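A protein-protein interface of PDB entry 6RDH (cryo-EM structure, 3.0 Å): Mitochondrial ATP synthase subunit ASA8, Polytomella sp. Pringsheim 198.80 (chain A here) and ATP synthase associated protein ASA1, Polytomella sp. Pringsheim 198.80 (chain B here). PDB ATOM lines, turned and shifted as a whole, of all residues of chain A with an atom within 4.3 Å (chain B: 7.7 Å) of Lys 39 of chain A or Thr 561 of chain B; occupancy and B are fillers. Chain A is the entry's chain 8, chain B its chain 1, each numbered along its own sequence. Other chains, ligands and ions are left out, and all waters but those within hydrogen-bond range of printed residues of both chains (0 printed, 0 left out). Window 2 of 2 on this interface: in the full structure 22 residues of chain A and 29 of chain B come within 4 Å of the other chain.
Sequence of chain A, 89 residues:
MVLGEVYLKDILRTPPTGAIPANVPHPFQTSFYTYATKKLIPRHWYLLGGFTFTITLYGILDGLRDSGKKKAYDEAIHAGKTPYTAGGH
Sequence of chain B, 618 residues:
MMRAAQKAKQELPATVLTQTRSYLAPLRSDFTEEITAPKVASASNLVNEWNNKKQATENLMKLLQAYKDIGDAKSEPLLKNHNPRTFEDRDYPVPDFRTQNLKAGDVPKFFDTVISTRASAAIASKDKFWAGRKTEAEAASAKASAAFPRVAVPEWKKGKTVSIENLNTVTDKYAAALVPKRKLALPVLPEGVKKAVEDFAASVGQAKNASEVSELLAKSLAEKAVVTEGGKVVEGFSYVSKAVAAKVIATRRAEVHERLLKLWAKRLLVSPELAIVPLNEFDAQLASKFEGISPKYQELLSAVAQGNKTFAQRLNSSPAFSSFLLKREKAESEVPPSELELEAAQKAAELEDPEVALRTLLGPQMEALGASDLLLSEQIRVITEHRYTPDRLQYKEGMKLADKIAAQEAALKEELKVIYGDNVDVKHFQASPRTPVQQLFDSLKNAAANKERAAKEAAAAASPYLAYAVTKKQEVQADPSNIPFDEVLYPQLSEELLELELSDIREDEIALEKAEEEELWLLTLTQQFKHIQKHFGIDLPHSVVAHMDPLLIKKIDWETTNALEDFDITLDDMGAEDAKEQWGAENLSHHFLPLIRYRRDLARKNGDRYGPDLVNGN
The side-chain carboxylate of Asp 557 of chain B lies close to a ring nitrogen (ND1) of His 26 of chain A, at 3.4 Å.
A ring nitrogen (NE2) of His 26 of chain A sits close to the side-chain hydroxyl (OG1) of Thr 561 of chain B.
The side-chain carboxylate (OE2) of Glu 565 of chain B is in salt-bridge range of the side-chain amino group (NZ) of Lys 39 of chain A (3.4 Å).
The backbone carbonyl oxygen (O) of Lys 39 of chain A lies within hydrogen-bond range of the backbone NH (N) of His 44 of chain A, at 3.4 Å.
O of Glu 559 of chain B is in hydrogen-bond range of N of Glu 565 of chain B (3.2 Å).
OG1 of Thr 560 of chain B is in hydrogen-bond range of O of Ile 556 of chain B (3.2 Å).
Among the printed residues, merely in contact across the chains: His 26 of chain A with Thr 560 of chain B (3.6 Å), Phe 28 of chain A with Thr 560 of chain B (3.8 Å), Phe 28 of chain A with Thr 561 of chain B (3.6 Å), Lys 38 of chain A with Thr 561 of chain B (3.9 Å), Lys 39 of chain A with Thr 560 of chain B (3.8 Å), Lys 39 of chain A with Thr 561 of chain B (3.99 Å), Lys 39 of chain A with Ala 563 of chain B (3.4 Å) and Arg 43 of chain A with Ala 563 of chain B (3.4 Å).
Printed residues of chain B within 4 Å of His 26 of chain A: Asp 557, Thr 560 and Thr 561.
Of the printed residues of chain B, Phe 28 of chain A touches Thr 560 and Thr 561.
Printed residues of chain B within 4 Å of Lys 39 of chain A: Thr 560, Thr 561, Ala 563 and Glu 565.
Of the printed residues of chain B, Arg 43 of chain A touches Ala 563 (3.4 Å).
Of the printed residues of chain A, Thr 561 of chain B touches His 26, Phe 28, Lys 38 and Lys 39.
Of the printed residues of chain A, Ala 563 of chain B touches Lys 39 and Arg 43.
Of the printed residues of chain A, Glu 565 of chain B touches Lys 39 (3.4 Å).
The nearest printed residue of chain B that does not touch Lys 39 of chain A is Asn 562 of chain B (5.4 Å).
Of the 11 printed residues of chain A, 5 touch a printed residue of chain B.
Hydrophobic or aromatic side chains of chain A within 4 Å of the printed part of chain B: His 26 and Phe 28.
Along chain A the printed residues that touch a printed residue of chain B span positions 26 to 43.
Of the 13 printed residues of chain B, 5 touch a printed residue of chain A.
Among the printed residues, 11 pairs touch across the chains.
Among the printed residues, Asp or Glu carboxylates within 4 Å of a Lys or Arg side-chain nitrogen of the other chain: Lys 39 of chain A with Glu 565 of chain B.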
ATOM      1  N   HIS A  26      16.146  -2.691  -4.244  1.00  0.00           N
ATOM      2  CA  HIS A  26      16.041  -3.973  -4.901  1.00  0.00           C
ATOM      3  C   HIS A  26      14.956  -3.898  -5.970  1.00  0.00           C
ATOM      4  O   HIS A  26      14.020  -3.107  -5.847  1.00  0.00           O
ATOM      5  CB  HIS A  26      15.707  -5.048  -3.878  1.00  0.00           C
ATOM      6  CG  HIS A  26      15.796  -6.435  -4.412  1.00  0.00           C
ATOM      7  ND1 HIS A  26      16.981  -7.002  -4.804  1.00  0.00           N
ATOM      8  CD2 HIS A  26      14.843  -7.361  -4.645  1.00  0.00           C
ATOM      9  CE1 HIS A  26      16.756  -8.219  -5.255  1.00  0.00           C
ATOM     10  NE2 HIS A  26      15.467  -8.464  -5.167  1.00  0.00           N
ATOM     11  N   PHE A  28      12.544  -5.813  -6.402  1.00  0.00           N
ATOM     12  CA  PHE A  28      11.243  -6.133  -5.839  1.00  0.00           C
ATOM     13  C   PHE A  28      10.662  -4.957  -5.083  1.00  0.00           C
ATOM     14  O   PHE A  28       9.443  -4.864  -4.940  1.00  0.00           O
ATOM     15  CB  PHE A  28      11.331  -7.319  -4.890  1.00  0.00           C
ATOM     16  CG  PHE A  28      11.722  -8.600  -5.539  1.00  0.00           C
ATOM     17  CD1 PHE A  28      11.534  -8.808  -6.884  1.00  0.00           C
ATOM     18  CD2 PHE A  28      12.276  -9.603  -4.792  1.00  0.00           C
ATOM     19  CE1 PHE A  28      11.904  -9.980  -7.462  1.00  0.00           C
ATOM     20  CE2 PHE A  28      12.636 -10.767  -5.372  1.00  0.00           C
ATOM     21  CZ  PHE A  28      12.443 -10.956  -6.707  1.00  0.00           C
ATOM     22  N   TYR A  35       8.295  -8.631  -8.746  1.00  0.00           N
ATOM     23  CA  TYR A  35       8.144  -9.619  -7.687  1.00  0.00           C
ATOM     24  C   TYR A  35       7.111 -10.659  -8.060  1.00  0.00           C
ATOM     25  O   TYR A  35       7.364 -11.861  -7.948  1.00  0.00           O
ATOM     26  CB  TYR A  35       7.750  -8.950  -6.379  1.00  0.00           C
ATOM     27  CG  TYR A  35       7.497  -9.952  -5.288  1.00  0.00           C
ATOM     28  CD1 TYR A  35       8.481 -10.844  -4.911  1.00  0.00           C
ATOM     29  CD2 TYR A  35       6.281 -10.017  -4.644  1.00  0.00           C
ATOM     30  CE1 TYR A  35       8.268 -11.759  -3.932  1.00  0.00           C
ATOM     31  CE2 TYR A  35       6.060 -10.941  -3.666  1.00  0.00           C
ATOM     32  CZ  TYR A  35       7.062 -11.808  -3.319  1.00  0.00           C
ATOM     33  OH  TYR A  35       6.863 -12.736  -2.339  1.00  0.00           O
ATOM     34  N   THR A  37       6.039 -11.653 -10.924  1.00  0.00           N
ATOM     35  CA  THR A  37       6.362 -12.513 -12.044  1.00  0.00           C
ATOM     36  C   THR A  37       7.686 -13.240 -11.894  1.00  0.00           C
ATOM     37  O   THR A  37       7.950 -14.157 -12.672  1.00  0.00           O
ATOM     38  CB  THR A  37       6.370 -11.694 -13.323  1.00  0.00           C
ATOM     39  OG1 THR A  37       7.186 -10.537 -13.132  1.00  0.00           O
ATOM     40  CG2 THR A  37       4.971 -11.248 -13.630  1.00  0.00           C
ATOM     41  N   LYS A  38       8.514 -12.879 -10.913  1.00  0.00           N
ATOM     42  CA  LYS A  38       9.793 -13.537 -10.723  1.00  0.00           C
ATOM     43  C   LYS A  38       9.878 -14.399  -9.478  1.00  0.00           C
ATOM     44  O   LYS A  38      10.623 -15.374  -9.485  1.00  0.00           O
ATOM     45  CB  LYS A  38      10.913 -12.500 -10.668  1.00  0.00           C
ATOM     46  CG  LYS A  38      11.279 -11.934 -12.007  1.00  0.00           C
ATOM     47  CD  LYS A  38      12.754 -12.100 -12.266  1.00  0.00           C
ATOM     48  CE  LYS A  38      13.071 -11.858 -13.721  1.00  0.00           C
ATOM     49  NZ  LYS A  38      14.499 -12.142 -14.015  1.00  0.00           N
ATOM     50  N   LYS A  39       9.155 -14.076  -8.409  1.00  0.00           N
ATOM     51  CA  LYS A  39       9.206 -14.910  -7.222  1.00  0.00           C
ATOM     52  C   LYS A  39       7.830 -15.337  -6.762  1.00  0.00           C
ATOM     53  O   LYS A  39       7.675 -16.461  -6.298  1.00  0.00           O
ATOM     54  CB  LYS A  39       9.905 -14.201  -6.073  1.00  0.00           C
ATOM     55  CG  LYS A  39      11.387 -14.386  -6.052  1.00  0.00           C
ATOM     56  CD  LYS A  39      11.929 -14.157  -4.680  1.00  0.00           C
ATOM     57  CE  LYS A  39      11.737 -15.355  -3.825  1.00  0.00           C
ATOM     58  NZ  LYS A  39      12.593 -16.451  -4.291  1.00  0.00           N
ATOM     59  N   LEU A  40       6.830 -14.468  -6.866  1.00  0.00           N
ATOM     60  CA  LEU A  40       5.553 -14.771  -6.227  1.00  0.00           C
ATOM     61  C   LEU A  40       4.808 -15.862  -6.967  1.00  0.00           C
ATOM     62  O   LEU A  40       4.258 -16.771  -6.348  1.00  0.00           O
ATOM     63  CB  LEU A  40       4.693 -13.526  -6.134  1.00  0.00           C
ATOM     64  CG  LEU A  40       3.376 -13.689  -5.408  1.00  0.00           C
ATOM     65  CD1 LEU A  40       3.638 -14.003  -3.974  1.00  0.00           C
ATOM     66  CD2 LEU A  40       2.593 -12.427  -5.526  1.00  0.00           C
ATOM     67  N   ILE A  41       4.770 -15.791  -8.285  1.00  0.00           N
ATOM     68  CA  ILE A  41       4.171 -16.866  -9.064  1.00  0.00           C
ATOM     69  C   ILE A  41       5.137 -18.035  -9.277  1.00  0.00           C
ATOM     70  O   ILE A  41       4.717 -19.169  -9.031  1.00  0.00           O
ATOM     71  CB  ILE A  41       3.575 -16.309 -10.365  1.00  0.00           C
ATOM     72  CG1 ILE A  41       2.322 -15.515 -10.026  1.00  0.00           C
ATOM     73  CG2 ILE A  41       3.233 -17.411 -11.325  1.00  0.00           C
ATOM     74  CD1 ILE A  41       1.844 -14.667 -11.135  1.00  0.00           C
ATOM     75  N   PRO A  42       6.411 -17.876  -9.685  1.00  0.00           N
ATOM     76  CA  PRO A  42       7.232 -19.082  -9.894  1.00  0.00           C
ATOM     77  C   PRO A  42       7.660 -19.815  -8.635  1.00  0.00           C
ATOM     78  O   PRO A  42       8.072 -20.974  -8.746  1.00  0.00           O
ATOM     79  CB  PRO A  42       8.451 -18.547 -10.644  1.00  0.00           C
ATOM     80  CG  PRO A  42       7.993 -17.342 -11.256  1.00  0.00           C
ATOM     81  CD  PRO A  42       7.127 -16.722 -10.259  1.00  0.00           C
ATOM     82  N   ARG A  43       7.596 -19.210  -7.455  1.00  0.00           N
ATOM     83  CA  ARG A  43       8.027 -19.897  -6.246  1.00  0.00           C
ATOM     84  C   ARG A  43       6.946 -20.057  -5.195  1.00  0.00           C
ATOM     85  O   ARG A  43       7.000 -21.019  -4.432  1.00  0.00           O
ATOM     86  CB  ARG A  43       9.212 -19.176  -5.594  1.00  0.00           C
ATOM     87  CG  ARG A  43      10.354 -18.887  -6.514  1.00  0.00           C
ATOM     88  CD  ARG A  43      11.140 -20.142  -6.780  1.00  0.00           C
ATOM     89  NE  ARG A  43      12.043 -20.458  -5.686  1.00  0.00           N
ATOM     90  CZ  ARG A  43      12.400 -21.690  -5.361  1.00  0.00           C
ATOM     91  NH1 ARG A  43      11.916 -22.713  -6.035  1.00  0.00           N
ATOM     92  NH2 ARG A  43      13.231 -21.898  -4.354  1.00  0.00           N
ATOM     93  N   HIS A  44       5.973 -19.152  -5.124  1.00  0.00           N
ATOM     94  CA  HIS A  44       4.988 -19.157  -4.054  1.00  0.00           C
ATOM     95  C   HIS A  44       3.588 -19.469  -4.553  1.00  0.00           C
ATOM     96  O   HIS A  44       2.608 -19.164  -3.864  1.00  0.00           O
ATOM     97  CB  HIS A  44       4.976 -17.818  -3.329  1.00  0.00           C
ATOM     98  CG  HIS A  44       6.311 -17.390  -2.816  1.00  0.00           C
ATOM     99  ND1 HIS A  44       7.225 -18.272  -2.292  1.00  0.00           N
ATOM    100  CD2 HIS A  44       6.883 -16.169  -2.746  1.00  0.00           C
ATOM    101  CE1 HIS A  44       8.306 -17.613  -1.922  1.00  0.00           C
ATOM    102  NE2 HIS A  44       8.123 -16.335  -2.186  1.00  0.00           N
ATOM    103  N   LYS B 554      24.698  -5.327  -6.682  1.00  0.00           N
ATOM    104  CA  LYS B 554      24.026  -5.805  -7.887  1.00  0.00           C
ATOM    105  C   LYS B 554      24.014  -7.326  -7.973  1.00  0.00           C
ATOM    106  O   LYS B 554      22.985  -7.925  -8.299  1.00  0.00           O
ATOM    107  CB  LYS B 554      24.705  -5.211  -9.107  1.00  0.00           C
ATOM    108  CG  LYS B 554      24.238  -5.766 -10.396  1.00  0.00           C
ATOM    109  CD  LYS B 554      24.966  -5.149 -11.529  1.00  0.00           C
ATOM    110  CE  LYS B 554      24.307  -5.525 -12.801  1.00  0.00           C
ATOM    111  NZ  LYS B 554      25.032  -4.939 -13.939  1.00  0.00           N
ATOM    112  N   LYS B 555      25.129  -7.969  -7.646  1.00  0.00           N
ATOM    113  CA  LYS B 555      25.186  -9.425  -7.698  1.00  0.00           C
ATOM    114  C   LYS B 555      24.375 -10.069  -6.583  1.00  0.00           C
ATOM    115  O   LYS B 555      23.734 -11.107  -6.789  1.00  0.00           O
ATOM    116  CB  LYS B 555      26.627  -9.879  -7.620  1.00  0.00           C
ATOM    117  CG  LYS B 555      27.436  -9.426  -8.771  1.00  0.00           C
ATOM    118  CD  LYS B 555      28.874  -9.637  -8.504  1.00  0.00           C
ATOM    119  CE  LYS B 555      29.664  -9.104  -9.628  1.00  0.00           C
ATOM    120  NZ  LYS B 555      31.051  -9.570  -9.570  1.00  0.00           N
ATOM    121  N   ILE B 556      24.388  -9.469  -5.397  1.00  0.00           N
ATOM    122  CA  ILE B 556      23.589  -9.980  -4.291  1.00  0.00           C
ATOM    123  C   ILE B 556      22.104  -9.830  -4.592  1.00  0.00           C
ATOM    124  O   ILE B 556      21.303 -10.731  -4.313  1.00  0.00           O
ATOM    125  CB  ILE B 556      24.008  -9.259  -2.999  1.00  0.00           C
ATOM    126  CG1 ILE B 556      25.371  -9.749  -2.549  1.00  0.00           C
ATOM    127  CG2 ILE B 556      23.030  -9.475  -1.907  1.00  0.00           C
ATOM    128  CD1 ILE B 556      25.983  -8.891  -1.535  1.00  0.00           C
ATOM    129  N   ASP B 557      21.721  -8.727  -5.232  1.00  0.00           N
ATOM    130  CA  ASP B 557      20.344  -8.556  -5.664  1.00  0.00           C
ATOM    131  C   ASP B 557      19.979  -9.498  -6.799  1.00  0.00           C
ATOM    132  O   ASP B 557      18.807  -9.829  -6.960  1.00  0.00           O
ATOM    133  CB  ASP B 557      20.116  -7.118  -6.089  1.00  0.00           C
ATOM    134  CG  ASP B 557      20.115  -6.177  -4.929  1.00  0.00           C
ATOM    135  OD1 ASP B 557      20.235  -6.662  -3.794  1.00  0.00           O
ATOM    136  OD2 ASP B 557      19.995  -4.956  -5.140  1.00  0.00           O
ATOM    137  N   TRP B 558      20.947  -9.925  -7.606  1.00  0.00           N
ATOM    138  CA  TRP B 558      20.662 -10.988  -8.564  1.00  0.00           C
ATOM    139  C   TRP B 558      20.353 -12.288  -7.852  1.00  0.00           C
ATOM    140  O   TRP B 558      19.483 -13.043  -8.287  1.00  0.00           O
ATOM    141  CB  TRP B 558      21.829 -11.196  -9.524  1.00  0.00           C
ATOM    142  CG  TRP B 558      21.514 -12.152 -10.627  1.00  0.00           C
ATOM    143  CD1 TRP B 558      21.038 -11.839 -11.848  1.00  0.00           C
ATOM    144  CD2 TRP B 558      21.642 -13.581 -10.604  1.00  0.00           C
ATOM    145  NE1 TRP B 558      20.853 -12.971 -12.590  1.00  0.00           N
ATOM    146  CE2 TRP B 558      21.218 -14.053 -11.840  1.00  0.00           C
ATOM    147  CE3 TRP B 558      22.073 -14.502  -9.651  1.00  0.00           C
ATOM    148  CZ2 TRP B 558      21.213 -15.392 -12.152  1.00  0.00           C
ATOM    149  CZ3 TRP B 558      22.059 -15.825  -9.963  1.00  0.00           C
ATOM    150  CH2 TRP B 558      21.636 -16.261 -11.197  1.00  0.00           C
ATOM    151  N   GLU B 559      21.085 -12.592  -6.786  1.00  0.00           N
ATOM    152  CA  GLU B 559      20.808 -13.819  -6.042  1.00  0.00           C
ATOM    153  C   GLU B 559      19.460 -13.762  -5.343  1.00  0.00           C
ATOM    154  O   GLU B 559      18.793 -14.786  -5.195  1.00  0.00           O
ATOM    155  CB  GLU B 559      21.888 -14.076  -5.012  1.00  0.00           C
ATOM    156  CG  GLU B 559      23.218 -14.297  -5.594  1.00  0.00           C
ATOM    157  CD  GLU B 559      24.151 -14.971  -4.645  1.00  0.00           C
ATOM    158  OE1 GLU B 559      23.684 -15.429  -3.593  1.00  0.00           O
ATOM    159  OE2 GLU B 559      25.352 -15.047  -4.943  1.00  0.00           O
ATOM    160  N   THR B 560      19.056 -12.586  -4.879  1.00  0.00           N
ATOM    161  CA  THR B 560      17.737 -12.467  -4.265  1.00  0.00           C
ATOM    162  C   THR B 560      16.633 -12.523  -5.316  1.00  0.00           C
ATOM    163  O   THR B 560      15.600 -13.159  -5.098  1.00  0.00           O
ATOM    164  CB  THR B 560      17.649 -11.180  -3.455  1.00  0.00           C
ATOM    165  OG1 THR B 560      18.717 -11.141  -2.509  1.00  0.00           O
ATOM    166  CG2 THR B 560      16.370 -11.116  -2.707  1.00  0.00           C
ATOM    167  N   THR B 561      16.847 -11.886  -6.468  1.00  0.00           N
ATOM    168  CA  THR B 561      15.846 -11.859  -7.531  1.00  0.00           C
ATOM    169  C   THR B 561      15.621 -13.239  -8.122  1.00  0.00           C
ATOM    170  O   THR B 561      14.489 -13.609  -8.443  1.00  0.00           O
ATOM    171  CB  THR B 561      16.283 -10.895  -8.632  1.00  0.00           C
ATOM    172  OG1 THR B 561      16.722  -9.671  -8.049  1.00  0.00           O
ATOM    173  CG2 THR B 561      15.151 -10.591  -9.556  1.00  0.00           C
ATOM    174  N   ASN B 562      16.686 -14.017  -8.268  1.00  0.00           N
ATOM    175  CA  ASN B 562      16.616 -15.305  -8.935  1.00  0.00           C
ATOM    176  C   ASN B 562      16.568 -16.463  -7.960  1.00  0.00           C
ATOM    177  O   ASN B 562      17.155 -17.511  -8.230  1.00  0.00           O
ATOM    178  CB  ASN B 562      17.786 -15.455  -9.889  1.00  0.00           C
ATOM    179  CG  ASN B 562      17.738 -14.447 -10.987  1.00  0.00           C
ATOM    180  OD1 ASN B 562      17.438 -13.288 -10.761  1.00  0.00           O
ATOM    181  ND2 ASN B 562      17.990 -14.888 -12.197  1.00  0.00           N
ATOM    182  N   ALA B 563      15.909 -16.265  -6.816  1.00  0.00           N
ATOM    183  CA  ALA B 563      15.519 -17.300  -5.862  1.00  0.00           C
ATOM    184  C   ALA B 563      16.696 -18.050  -5.270  1.00  0.00           C
ATOM    185  O   ALA B 563      16.537 -19.173  -4.797  1.00  0.00           O
ATOM    186  CB  ALA B 563      14.539 -18.288  -6.490  1.00  0.00           C
ATOM    187  N   LEU B 564      17.876 -17.457  -5.279  1.00  0.00           N
ATOM    188  CA  LEU B 564      19.076 -18.087  -4.762  1.00  0.00           C
ATOM    189  C   LEU B 564      19.574 -17.345  -3.541  1.00  0.00           C
ATOM    190  O   LEU B 564      20.769 -17.217  -3.313  1.00  0.00           O
ATOM    191  CB  LEU B 564      20.158 -18.149  -5.828  1.00  0.00           C
ATOM    192  CG  LEU B 564      19.879 -19.045  -7.021  1.00  0.00           C
ATOM    193  CD1 LEU B 564      20.878 -18.741  -8.099  1.00  0.00           C
ATOM    194  CD2 LEU B 564      19.975 -20.483  -6.601  1.00  0.00           C
ATOM    195  N   GLU B 565      18.642 -16.852  -2.733  1.00  0.00           N
ATOM    196  CA  GLU B 565      18.979 -16.101  -1.536  1.00  0.00           C
ATOM    197  C   GLU B 565      19.600 -16.970  -0.464  1.00  0.00           C
ATOM    198  O   GLU B 565      20.228 -16.449   0.456  1.00  0.00           O
ATOM    199  CB  GLU B 565      17.713 -15.449  -1.025  1.00  0.00           C
ATOM    200  CG  GLU B 565      16.618 -16.450  -0.917  1.00  0.00           C
ATOM    201  CD  GLU B 565      15.292 -15.894  -1.309  1.00  0.00           C
ATOM    202  OE1 GLU B 565      15.212 -14.674  -1.550  1.00  0.00           O
ATOM    203  OE2 GLU B 565      14.335 -16.685  -1.425  1.00  0.00           O
ATOM    204  N   ASP B 566      19.433 -18.278  -0.559  1.00  0.00           N
ATOM    205  CA  ASP B 566      20.067 -19.223   0.336  1.00  0.00           C
ATOM    206  C   ASP B 566      21.169 -19.998  -0.366  1.00  0.00           C
ATOM    207  O   ASP B 566      21.383 -21.171  -0.069  1.00  0.00           O
ATOM    208  CB  ASP B 566      19.028 -20.184   0.897  1.00  0.00           C
ATOM    209  CG  ASP B 566      18.260 -20.907  -0.189  1.00  0.00           C
ATOM    210  OD1 ASP B 566      17.857 -20.270  -1.176  1.00  0.00           O
ATOM    211  OD2 ASP B 566      18.056 -22.125  -0.057  1.00  0.00           O
